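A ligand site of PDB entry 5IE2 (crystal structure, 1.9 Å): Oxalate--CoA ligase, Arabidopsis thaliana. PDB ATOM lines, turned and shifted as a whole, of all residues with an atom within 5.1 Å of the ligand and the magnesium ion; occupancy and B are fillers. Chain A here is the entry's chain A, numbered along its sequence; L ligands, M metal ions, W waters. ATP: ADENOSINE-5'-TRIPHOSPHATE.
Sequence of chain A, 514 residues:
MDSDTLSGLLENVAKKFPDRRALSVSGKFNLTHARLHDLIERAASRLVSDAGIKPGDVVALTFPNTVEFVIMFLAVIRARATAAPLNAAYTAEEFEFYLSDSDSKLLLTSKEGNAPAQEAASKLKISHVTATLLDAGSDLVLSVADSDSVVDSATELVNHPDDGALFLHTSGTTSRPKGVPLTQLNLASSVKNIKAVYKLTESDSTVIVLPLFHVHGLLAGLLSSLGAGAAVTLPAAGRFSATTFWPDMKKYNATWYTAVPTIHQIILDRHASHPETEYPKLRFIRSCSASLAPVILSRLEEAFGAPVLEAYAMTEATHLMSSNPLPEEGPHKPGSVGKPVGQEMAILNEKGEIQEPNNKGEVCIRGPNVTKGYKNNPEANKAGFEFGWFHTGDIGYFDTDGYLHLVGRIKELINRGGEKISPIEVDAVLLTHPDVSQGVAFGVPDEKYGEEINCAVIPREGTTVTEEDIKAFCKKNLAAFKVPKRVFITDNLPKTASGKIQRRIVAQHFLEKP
N of Ser 175 touches O1G of the ligand, 3.99 Å away. Ala 290 touches the ligand. Tyr 312 touches the ligand (CA to N7, 3.7 Å). O of Ala 313 touches C8 of the ligand, at 3.2 Å. Met 314 touches the ligand (CB to C5', 3.4 Å). Val 337 touches the ligand (CG1 to N6, 3.4 Å). Leu 406 touches the ligand. Of the 29 residues printed, 21 come within 4 Å of the ligand.
No residue comes within 4 Å of the magnesium ion. The nearest printed residue that does not touch the magnesium ion is Arg 409 (4.2 Å).
The side-chain hydroxyl (OH) of Tyr 312 is in hydrogen-bond range of the side-chain carboxylate (OD2) of Asp 394 (2.6 Å). The backbone NH (N) of Asp 394 sits at hydrogen-bond distance from the side-chain hydroxyl (OG1) of Thr 392 (3.1 Å). The backbone carbonyl oxygen of Ala 311 is in hydrogen-bond range of the side-chain sulfur of Cys 288. The side-chain hydroxyl (OG1) of Thr 170 lies within hydrogen-bond range of the backbone NH (N) of Lys 178, at 2.8 Å. NZ of Lys 500 sits at hydrogen-bond distance from O of Ser 289, 2.8 Å away. The backbone NH (N) of Leu 292 is in hydrogen-bond range of the side-chain carboxylate (OE2) of Glu 310. N of Ala 313 sits close to SG of Cys 288 (3.7 Å). OG1 of Thr 392 sits at hydrogen-bond distance from OH of Tyr 312, 3.3 Å away.
Water W2 lies within hydrogen-bond range of the side-chain carboxylate (OE1) of Glu 316 and an oxygen (O1A) of the ligand. Water W7 lies within hydrogen-bond range of O1G of the ligand (2.6 Å), OG1 of Thr 174 (3.0 Å) and NH1 of Arg 409 (3.5 Å). Water W1 lies within hydrogen-bond range of an oxygen (O2G) of the ligand, the backbone carbonyl oxygen of Arg 176 and the side-chain hydroxyl of Thr 170. Water W4 lies within hydrogen-bond range of a nitrogen (N1) of the ligand (2.8 Å) and the side-chain carboxylate of Glu 310 (3.1 Å).
The backbone NH (N) of Thr 173 lies within hydrogen-bond range of an oxygen (O3B) of the ligand, 3.3 Å away. O1B of the ligand lies within hydrogen-bond range of OG1 of Thr 173, 2.6 Å away. N of Gly 172 is in hydrogen-bond range of O2G of the ligand (2.6 Å). The side-chain carboxylate (OD1) of Asp 394 lies within hydrogen-bond range of an oxygen (O2') of the ligand (2.7 Å). The guanidinium group (NH2) of Arg 409 lies within salt-bridge range of an oxygen (O1B) of the ligand (3.1 Å). The backbone carbonyl oxygen of Ala 311 is in hydrogen-bond range of a nitrogen (N6) of the ligand (2.9 Å). O1A of the ligand sits at hydrogen-bond distance from N of Thr 315. An oxygen (O1A) of the ligand sits at hydrogen-bond distance from the side-chain hydroxyl of Thr 315, at 3.0 Å. O1G of the ligand is in hydrogen-bond range of N of Thr 174. An oxygen (O1G) of the ligand is in hydrogen-bond range of the side-chain hydroxyl (OG1) of Thr 174 (3.2 Å). The side-chain hydroxyl of Thr 170 is in hydrogen-bond range of an oxygen (O2G) of the ligand, at 2.9 Å. N of Ser 171 lies within hydrogen-bond range of O3B of the ligand, at 3.3 Å. OG of Ser 171 sits at hydrogen-bond distance from O2A of the ligand. A ring nitrogen (NE2) of His 214 sits at hydrogen-bond distance from an oxygen (O2A) of the ligand, 3.0 Å away. O1B of the ligand is in salt-bridge range of NZ of Lys 500, at 3.5 Å. N6 of the ligand sits at hydrogen-bond distance from OE2 of Glu 310 (3.1 Å). A nitrogen (N7) of the ligand lies within hydrogen-bond range of the backbone NH of Ser 289 (3.2 Å). A nitrogen (N1) of the ligand is in hydrogen-bond range of the backbone NH of Ser 291 (3.2 Å).
The magnesium ion is bound by O3G of the ligand. Water W6 is bound to the magnesium ion (2.1 Å). The magnesium ion is bound by O2B of the ligand (2.1 Å). The magnesium ion is bound by water W2 (2.2 Å). The magnesium ion is bound by water W7 (2.2 Å). The magnesium ion is bound by water W3, 2.3 Å away.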
ATOM      1  N   THR A 170      -2.219   1.890  19.350  1.00  0.00           N
ATOM      2  CA  THR A 170      -0.894   1.395  19.707  1.00  0.00           C
ATOM      3  C   THR A 170      -0.573   1.616  21.207  1.00  0.00           C
ATOM      4  O   THR A 170      -1.230   2.433  21.853  1.00  0.00           O
ATOM      5  CB  THR A 170       0.159   2.020  18.847  1.00  0.00           C
ATOM      6  OG1 THR A 170       0.012   3.451  18.910  1.00  0.00           O
ATOM      7  CG2 THR A 170      -0.002   1.520  17.400  1.00  0.00           C
ATOM      8  N   SER A 171       0.383   0.852  21.757  1.00  0.00           N
ATOM      9  CA  SER A 171       0.668   0.853  23.204  1.00  0.00           C
ATOM     10  C   SER A 171       1.181   2.198  23.798  1.00  0.00           C
ATOM     11  O   SER A 171       1.244   2.325  25.016  1.00  0.00           O
ATOM     12  CB  SER A 171       1.679  -0.249  23.528  1.00  0.00           C
ATOM     13  OG  SER A 171       1.112  -1.540  23.341  1.00  0.00           O
ATOM     14  N   GLY A 172       1.556   3.189  22.976  1.00  0.00           N
ATOM     15  CA  GLY A 172       1.954   4.492  23.503  1.00  0.00           C
ATOM     16  C   GLY A 172       3.425   4.575  23.948  1.00  0.00           C
ATOM     17  O   GLY A 172       3.856   5.491  24.689  1.00  0.00           O
ATOM     18  N   THR A 173       4.227   3.629  23.471  1.00  0.00           N
ATOM     19  CA  THR A 173       5.611   3.524  23.866  1.00  0.00           C
ATOM     20  C   THR A 173       6.495   4.716  23.412  1.00  0.00           C
ATOM     21  O   THR A 173       7.215   5.294  24.221  1.00  0.00           O
ATOM     22  CB  THR A 173       6.203   2.194  23.348  1.00  0.00           C
ATOM     23  OG1 THR A 173       5.374   1.091  23.786  1.00  0.00           O
ATOM     24  CG2 THR A 173       7.664   2.010  23.851  1.00  0.00           C
ATOM     25  N   THR A 174       6.478   5.063  22.134  1.00  0.00           N
ATOM     26  CA  THR A 174       7.338   6.145  21.657  1.00  0.00           C
ATOM     27  C   THR A 174       6.525   7.340  21.146  1.00  0.00           C
ATOM     28  O   THR A 174       7.057   8.223  20.473  1.00  0.00           O
ATOM     29  CB  THR A 174       8.350   5.701  20.543  1.00  0.00           C
ATOM     30  OG1 THR A 174       7.654   5.020  19.491  1.00  0.00           O
ATOM     31  CG2 THR A 174       9.417   4.791  21.111  1.00  0.00           C
ATOM     32  N   SER A 175       5.227   7.314  21.424  1.00  0.00           N
ATOM     33  CA  SER A 175       4.319   8.354  20.939  1.00  0.00           C
ATOM     34  C   SER A 175       3.021   8.326  21.725  1.00  0.00           C
ATOM     35  O   SER A 175       2.851   7.483  22.620  1.00  0.00           O
ATOM     36  CB  SER A 175       4.046   8.171  19.439  1.00  0.00           C
ATOM     37  OG  SER A 175       4.990   8.894  18.662  1.00  0.00           O
ATOM     38  N   ARG A 176       2.108   9.228  21.386  1.00  0.00           N
ATOM     39  CA  ARG A 176       0.721   9.136  21.850  1.00  0.00           C
ATOM     40  C   ARG A 176       0.060   8.057  20.985  1.00  0.00           C
ATOM     41  O   ARG A 176       0.232   8.097  19.751  1.00  0.00           O
ATOM     42  CB  ARG A 176      -0.004  10.482  21.699  1.00  0.00           C
ATOM     43  CG  ARG A 176       0.628  11.401  20.648  1.00  0.00           C
ATOM     44  CD  ARG A 176       0.226  12.850  20.803  1.00  0.00           C
ATOM     45  NE  ARG A 176       1.084  13.755  20.035  1.00  0.00           N
ATOM     46  CZ  ARG A 176       2.200  14.322  20.524  1.00  0.00           C
ATOM     47  NH1 ARG A 176       2.581  14.066  21.768  1.00  0.00           N
ATOM     48  NH2 ARG A 176       2.919  15.137  19.771  1.00  0.00           N
ATOM     49  N   PRO A 177      -0.646   7.086  21.628  1.00  0.00           N
ATOM     50  CA  PRO A 177      -1.217   5.928  20.898  1.00  0.00           C
ATOM     51  C   PRO A 177      -1.940   6.361  19.598  1.00  0.00           C
ATOM     52  O   PRO A 177      -2.682   7.365  19.590  1.00  0.00           O
ATOM     53  CB  PRO A 177      -2.201   5.319  21.918  1.00  0.00           C
ATOM     54  CG  PRO A 177      -1.535   5.634  23.286  1.00  0.00           C
ATOM     55  CD  PRO A 177      -0.900   7.002  23.086  1.00  0.00           C
ATOM     56  N   LYS A 178      -1.635   5.658  18.501  1.00  0.00           N
ATOM     57  CA  LYS A 178      -2.268   5.933  17.195  1.00  0.00           C
ATOM     58  C   LYS A 178      -3.423   4.953  16.980  1.00  0.00           C
ATOM     59  O   LYS A 178      -3.273   3.811  17.380  1.00  0.00           O
ATOM     60  CB  LYS A 178      -1.241   5.798  16.059  1.00  0.00           C
ATOM     61  CG  LYS A 178      -0.270   6.968  15.854  1.00  0.00           C
ATOM     62  CD  LYS A 178       0.773   6.583  14.806  1.00  0.00           C
ATOM     63  CE  LYS A 178       1.433   7.780  14.171  1.00  0.00           C
ATOM     64  NZ  LYS A 178       1.672   8.935  15.089  1.00  0.00           N
ATOM     65  N   HIS A 214      -5.268  -6.577  23.419  1.00  0.00           N
ATOM     66  CA  HIS A 214      -4.032  -6.254  22.640  1.00  0.00           C
ATOM     67  C   HIS A 214      -3.872  -7.360  21.580  1.00  0.00           C
ATOM     68  O   HIS A 214      -4.371  -8.495  21.785  1.00  0.00           O
ATOM     69  CB  HIS A 214      -2.794  -6.146  23.579  1.00  0.00           C
ATOM     70  CG  HIS A 214      -1.482  -5.918  22.874  1.00  0.00           C
ATOM     71  ND1 HIS A 214      -0.748  -6.939  22.276  1.00  0.00           N
ATOM     72  CD2 HIS A 214      -0.779  -4.777  22.648  1.00  0.00           C
ATOM     73  CE1 HIS A 214       0.333  -6.435  21.699  1.00  0.00           C
ATOM     74  NE2 HIS A 214       0.348  -5.121  21.920  1.00  0.00           N
ATOM     75  N   CYS A 288       6.981 -12.888  22.303  1.00  0.00           N
ATOM     76  CA  CYS A 288       6.825 -11.797  21.303  1.00  0.00           C
ATOM     77  C   CYS A 288       6.616 -10.506  22.052  1.00  0.00           C
ATOM     78  O   CYS A 288       6.433 -10.528  23.292  1.00  0.00           O
ATOM     79  CB  CYS A 288       5.649 -12.139  20.332  1.00  0.00           C
ATOM     80  SG  CYS A 288       5.586 -11.076  18.892  1.00  0.00           S
ATOM     81  N   SER A 289       6.679  -9.365  21.333  1.00  0.00           N
ATOM     82  CA  SER A 289       6.241  -8.004  21.748  1.00  0.00           C
ATOM     83  C   SER A 289       7.334  -7.151  22.370  1.00  0.00           C
ATOM     84  O   SER A 289       7.195  -5.926  22.377  1.00  0.00           O
ATOM     85  CB  SER A 289       5.053  -7.994  22.742  1.00  0.00           C
ATOM     86  OG  SER A 289       3.939  -8.762  22.233  1.00  0.00           O
ATOM     87  N   ALA A 290       8.388  -7.779  22.918  1.00  0.00           N
ATOM     88  CA  ALA A 290       9.532  -7.062  23.466  1.00  0.00           C
ATOM     89  C   ALA A 290      10.684  -8.024  23.389  1.00  0.00           C
ATOM     90  O   ALA A 290      10.415  -9.235  23.356  1.00  0.00           O
ATOM     91  CB  ALA A 290       9.266  -6.623  24.946  1.00  0.00           C
ATOM     92  N   SER A 291      11.936  -7.562  23.406  1.00  0.00           N
ATOM     93  CA  SER A 291      13.047  -8.515  23.168  1.00  0.00           C
ATOM     94  C   SER A 291      13.151  -9.531  24.267  1.00  0.00           C
ATOM     95  O   SER A 291      13.037  -9.195  25.482  1.00  0.00           O
ATOM     96  CB  SER A 291      14.397  -7.833  22.959  1.00  0.00           C
ATOM     97  OG  SER A 291      14.688  -7.072  24.082  1.00  0.00           O
ATOM     98  N   LEU A 292      13.326 -10.785  23.874  1.00  0.00           N
ATOM     99  CA  LEU A 292      13.588 -11.889  24.814  1.00  0.00           C
ATOM    100  C   LEU A 292      15.119 -12.034  24.979  1.00  0.00           C
ATOM    101  O   LEU A 292      15.814 -12.418  24.034  1.00  0.00           O
ATOM    102  CB  LEU A 292      13.040 -13.242  24.299  1.00  0.00           C
ATOM    103  CG  LEU A 292      13.228 -14.460  25.212  1.00  0.00           C
ATOM    104  CD1 LEU A 292      12.340 -14.338  26.428  1.00  0.00           C
ATOM    105  CD2 LEU A 292      12.864 -15.778  24.486  1.00  0.00           C
ATOM    106  N   GLU A 310      11.108 -17.086  19.403  1.00  0.00           N
ATOM    107  CA  GLU A 310      10.817 -15.662  19.492  1.00  0.00           C
ATOM    108  C   GLU A 310      10.275 -15.108  18.170  1.00  0.00           C
ATOM    109  O   GLU A 310      10.761 -15.468  17.083  1.00  0.00           O
ATOM    110  CB  GLU A 310      12.098 -14.894  19.870  1.00  0.00           C
ATOM    111  CG  GLU A 310      11.772 -13.447  20.259  1.00  0.00           C
ATOM    112  CD  GLU A 310      12.972 -12.627  20.679  1.00  0.00           C
ATOM    113  OE1 GLU A 310      14.137 -13.072  20.534  1.00  0.00           O
ATOM    114  OE2 GLU A 310      12.737 -11.477  21.150  1.00  0.00           O
ATOM    115  N   ALA A 311       9.253 -14.282  18.289  1.00  0.00           N
ATOM    116  CA  ALA A 311       8.636 -13.640  17.127  1.00  0.00           C
ATOM    117  C   ALA A 311       8.696 -12.119  17.300  1.00  0.00           C
ATOM    118  O   ALA A 311       8.870 -11.636  18.421  1.00  0.00           O
ATOM    119  CB  ALA A 311       7.186 -14.079  16.959  1.00  0.00           C
ATOM    120  N   TYR A 312       8.469 -11.393  16.202  1.00  0.00           N
ATOM    121  CA  TYR A 312       8.430  -9.928  16.161  1.00  0.00           C
ATOM    122  C   TYR A 312       7.082  -9.516  15.559  1.00  0.00           C
ATOM    123  O   TYR A 312       6.640 -10.100  14.565  1.00  0.00           O
ATOM    124  CB  TYR A 312       9.609  -9.443  15.316  1.00  0.00           C
ATOM    125  CG  TYR A 312       9.581  -8.015  14.771  1.00  0.00           C
ATOM    126  CD1 TYR A 312       9.442  -6.908  15.624  1.00  0.00           C
ATOM    127  CD2 TYR A 312       9.857  -7.778  13.431  1.00  0.00           C
ATOM    128  CE1 TYR A 312       9.506  -5.566  15.128  1.00  0.00           C
ATOM    129  CE2 TYR A 312       9.943  -6.476  12.929  1.00  0.00           C
ATOM    130  CZ  TYR A 312       9.738  -5.394  13.761  1.00  0.00           C
ATOM    131  OH  TYR A 312       9.800  -4.127  13.233  1.00  0.00           O
ATOM    132  N   ALA A 313       6.400  -8.589  16.214  1.00  0.00           N
ATOM    133  CA  ALA A 313       5.013  -8.267  15.858  1.00  0.00           C
ATOM    134  C   ALA A 313       4.636  -6.843  16.231  1.00  0.00           C
ATOM    135  O   ALA A 313       5.291  -6.254  17.028  1.00  0.00           O
ATOM    136  CB  ALA A 313       4.036  -9.242  16.564  1.00  0.00           C
ATOM    137  N   MET A 314       3.589  -6.307  15.608  1.00  0.00           N
ATOM    138  CA  MET A 314       3.126  -4.964  15.994  1.00  0.00           C
ATOM    139  C   MET A 314       1.677  -4.811  15.595  1.00  0.00           C
ATOM    140  O   MET A 314       1.153  -5.523  14.729  1.00  0.00           O
ATOM    141  CB  MET A 314       4.032  -3.885  15.350  1.00  0.00           C
ATOM    142  CG  MET A 314       3.871  -3.736  13.823  1.00  0.00           C
ATOM    143  SD  MET A 314       5.199  -2.681  13.168  1.00  0.00           S
ATOM    144  CE  MET A 314       5.100  -1.168  14.146  1.00  0.00           C
ATOM    145  N   THR A 315       0.997  -3.861  16.239  1.00  0.00           N
ATOM    146  CA  THR A 315      -0.415  -3.687  16.005  1.00  0.00           C
ATOM    147  C   THR A 315      -0.693  -3.408  14.506  1.00  0.00           C
ATOM    148  O   THR A 315      -1.652  -3.910  13.980  1.00  0.00           O
ATOM    149  CB  THR A 315      -0.966  -2.500  16.858  1.00  0.00           C
ATOM    150  OG1 THR A 315      -0.714  -2.769  18.236  1.00  0.00           O
ATOM    151  CG2 THR A 315      -2.463  -2.336  16.676  1.00  0.00           C
ATOM    152  N   GLU A 316       0.142  -2.576  13.891  1.00  0.00           N
ATOM    153  CA  GLU A 316      -0.072  -2.205  12.476  1.00  0.00           C
ATOM    154  C   GLU A 316       0.070  -3.346  11.461  1.00  0.00           C
ATOM    155  O   GLU A 316      -0.376  -3.241  10.302  1.00  0.00           O
ATOM    156  CB  GLU A 316       0.906  -1.094  12.062  1.00  0.00           C
ATOM    157  CG  GLU A 316       0.665   0.254  12.691  1.00  0.00           C
ATOM    158  CD  GLU A 316       1.495   0.442  13.985  1.00  0.00           C
ATOM    159  OE1 GLU A 316       1.720  -0.562  14.699  1.00  0.00           O
ATOM    160  OE2 GLU A 316       1.925   1.581  14.249  1.00  0.00           O
ATOM    161  N   VAL A 337      14.705 -12.496  15.911  1.00  0.00           N
ATOM    162  CA  VAL A 337      13.284 -12.724  15.777  1.00  0.00           C
ATOM    163  C   VAL A 337      12.932 -13.465  14.458  1.00  0.00           C
ATOM    164  O   VAL A 337      11.775 -13.442  13.985  1.00  0.00           O
ATOM    165  CB  VAL A 337      12.489 -11.389  15.908  1.00  0.00           C
ATOM    166  CG1 VAL A 337      12.632 -10.835  17.286  1.00  0.00           C
ATOM    167  CG2 VAL A 337      12.998 -10.335  14.923  1.00  0.00           C
ATOM    168  N   THR A 392       8.325   0.587   9.949  1.00  0.00           N
ATOM    169  CA  THR A 392       7.966   0.157  11.333  1.00  0.00           C
ATOM    170  C   THR A 392       8.472   1.091  12.451  1.00  0.00           C
ATOM    171  O   THR A 392       7.975   1.017  13.571  1.00  0.00           O
ATOM    172  CB  THR A 392       8.488  -1.256  11.697  1.00  0.00           C
ATOM    173  OG1 THR A 392       9.934  -1.229  11.639  1.00  0.00           O
ATOM    174  CG2 THR A 392       7.987  -2.274  10.722  1.00  0.00           C
ATOM    175  N   ASP A 394      11.447   0.600  13.627  1.00  0.00           N
ATOM    176  CA  ASP A 394      12.451  -0.251  14.284  1.00  0.00           C
ATOM    177  C   ASP A 394      13.669  -0.358  13.408  1.00  0.00           C
ATOM    178  O   ASP A 394      13.557  -0.467  12.175  1.00  0.00           O
ATOM    179  CB  ASP A 394      11.897  -1.668  14.550  1.00  0.00           C
ATOM    180  CG  ASP A 394      10.660  -1.669  15.453  1.00  0.00           C
ATOM    181  OD1 ASP A 394      10.735  -1.039  16.546  1.00  0.00           O
ATOM    182  OD2 ASP A 394       9.596  -2.301  15.096  1.00  0.00           O
ATOM    183  N   LEU A 406      16.920  -7.410  15.795  1.00  0.00           N
ATOM    184  CA  LEU A 406      16.506  -6.037  16.116  1.00  0.00           C
ATOM    185  C   LEU A 406      17.522  -5.297  16.972  1.00  0.00           C
ATOM    186  O   LEU A 406      18.108  -5.849  17.916  1.00  0.00           O
ATOM    187  CB  LEU A 406      15.155  -6.064  16.817  1.00  0.00           C
ATOM    188  CG  LEU A 406      14.026  -6.528  15.908  1.00  0.00           C
ATOM    189  CD1 LEU A 406      12.816  -6.825  16.816  1.00  0.00           C
ATOM    190  CD2 LEU A 406      13.670  -5.554  14.808  1.00  0.00           C
ATOM    191  N   ARG A 409      14.021   0.482  18.712  1.00  0.00           N
ATOM    192  CA  ARG A 409      13.251   1.564  18.124  1.00  0.00           C
ATOM    193  C   ARG A 409      14.143   2.732  17.824  1.00  0.00           C
ATOM    194  O   ARG A 409      15.002   3.098  18.636  1.00  0.00           O
ATOM    195  CB  ARG A 409      12.134   1.996  19.048  1.00  0.00           C
ATOM    196  CG  ARG A 409      11.201   0.871  19.384  1.00  0.00           C
ATOM    197  CD  ARG A 409      10.520   1.179  20.694  1.00  0.00           C
ATOM    198  NE  ARG A 409       9.765   0.081  21.286  1.00  0.00           N
ATOM    199  CZ  ARG A 409       8.457  -0.075  21.107  1.00  0.00           C
ATOM    200  NH1 ARG A 409       7.801   0.781  20.317  1.00  0.00           N
ATOM    201  NH2 ARG A 409       7.826  -1.088  21.701  1.00  0.00           N
ATOM    202  N   ILE A 424      18.372  -2.685  24.012  1.00  0.00           N
ATOM    203  CA  ILE A 424      18.109  -4.147  23.944  1.00  0.00           C
ATOM    204  C   ILE A 424      19.344  -4.961  24.367  1.00  0.00           C
ATOM    205  O   ILE A 424      19.281  -5.892  25.206  1.00  0.00           O
ATOM    206  CB  ILE A 424      17.688  -4.550  22.490  1.00  0.00           C
ATOM    207  CG1 ILE A 424      16.274  -4.055  22.213  1.00  0.00           C
ATOM    208  CG2 ILE A 424      17.774  -6.098  22.259  1.00  0.00           C
ATOM    209  CD1 ILE A 424      15.771  -4.467  20.825  1.00  0.00           C
ATOM    210  N   LYS A 500       4.762  -4.608  28.876  1.00  0.00           N
ATOM    211  CA  LYS A 500       6.013  -3.961  28.429  1.00  0.00           C
ATOM    212  C   LYS A 500       6.482  -2.958  29.433  1.00  0.00           C
ATOM    213  O   LYS A 500       5.688  -2.151  29.916  1.00  0.00           O
ATOM    214  CB  LYS A 500       5.863  -3.198  27.102  1.00  0.00           C
ATOM    215  CG  LYS A 500       5.306  -3.924  25.910  1.00  0.00           C
ATOM    216  CD  LYS A 500       5.043  -2.892  24.763  1.00  0.00           C
ATOM    217  CE  LYS A 500       4.290  -3.512  23.552  1.00  0.00           C
ATOM    218  NZ  LYS A 500       5.233  -3.951  22.420  1.00  0.00           N
HETATM  219  PG  ATP L   1       3.543   2.870  20.041  1.00  0.00           P
HETATM  220  O1G ATP L   1       4.910   3.539  20.173  1.00  0.00           O
HETATM  221  O2G ATP L   1       2.430   3.712  20.559  1.00  0.00           O
HETATM  222  O3G ATP L   1       3.302   2.391  18.619  1.00  0.00           O
HETATM  223  PB  ATP L   1       4.279   0.136  20.625  1.00  0.00           P
HETATM  224  O1B ATP L   1       4.793  -0.547  21.877  1.00  0.00           O
HETATM  225  O2B ATP L   1       5.173   0.393  19.473  1.00  0.00           O
HETATM  226  O3B ATP L   1       3.524   1.545  20.999  1.00  0.00           O
HETATM  227  PA  ATP L   1       2.876  -2.332  19.822  1.00  0.00           P
HETATM  228  O1A ATP L   1       2.288  -2.443  18.416  1.00  0.00           O
HETATM  229  O2A ATP L   1       2.164  -2.939  20.968  1.00  0.00           O
HETATM  230  O3A ATP L   1       2.992  -0.761  20.159  1.00  0.00           O
HETATM  231  O5' ATP L   1       4.403  -2.815  19.758  1.00  0.00           O
HETATM  232  C5' ATP L   1       5.106  -3.155  18.543  1.00  0.00           C
HETATM  233  C4' ATP L   1       6.596  -2.869  18.801  1.00  0.00           C
HETATM  234  O4' ATP L   1       7.093  -3.811  19.770  1.00  0.00           O
HETATM  235  C3' ATP L   1       7.458  -3.148  17.607  1.00  0.00           C
HETATM  236  O3' ATP L   1       7.430  -2.037  16.727  1.00  0.00           O
HETATM  237  C2' ATP L   1       8.824  -3.364  18.219  1.00  0.00           C
HETATM  238  O2' ATP L   1       9.371  -2.092  18.615  1.00  0.00           O
HETATM  239  C1' ATP L   1       8.460  -4.072  19.503  1.00  0.00           C
HETATM  240  N9  ATP L   1       8.629  -5.540  19.412  1.00  0.00           N
HETATM  241  C8  ATP L   1       7.713  -6.469  19.106  1.00  0.00           C
HETATM  242  N7  ATP L   1       8.300  -7.705  19.161  1.00  0.00           N
HETATM  243  C5  ATP L   1       9.597  -7.515  19.547  1.00  0.00           C
HETATM  244  C6  ATP L   1      10.756  -8.396  19.826  1.00  0.00           C
HETATM  245  N6  ATP L   1      10.612  -9.762  19.753  1.00  0.00           N
HETATM  246  N1  ATP L   1      11.910  -7.791  20.194  1.00  0.00           N
HETATM  247  C2  ATP L   1      12.018  -6.451  20.314  1.00  0.00           C
HETATM  248  N3  ATP L   1      11.008  -5.583  20.069  1.00  0.00           N
HETATM  249  C4  ATP L   1       9.798  -6.087  19.696  1.00  0.00           C
HETATM  250 MG    MG M   1       4.651   1.304  17.613  1.00  0.00          MG
HETATM  251  O   HOH W   1       2.021   5.856  19.162  1.00  0.00           O
HETATM  252  O   HOH W   2       3.171  -0.220  16.995  1.00  0.00           O
HETATM  253  O   HOH W   3       4.000   2.373  15.699  1.00  0.00           O
HETATM  254  O   HOH W   4      14.362  -9.144  19.874  1.00  0.00           O
HETATM  255  O   HOH W   5      11.792  -2.966  20.056  1.00  0.00           O
HETATM  256  O   HOH W   6       6.374   0.365  16.882  1.00  0.00           O
HETATM  257  O   HOH W   7       6.231   2.846  17.985  1.00  0.00           O
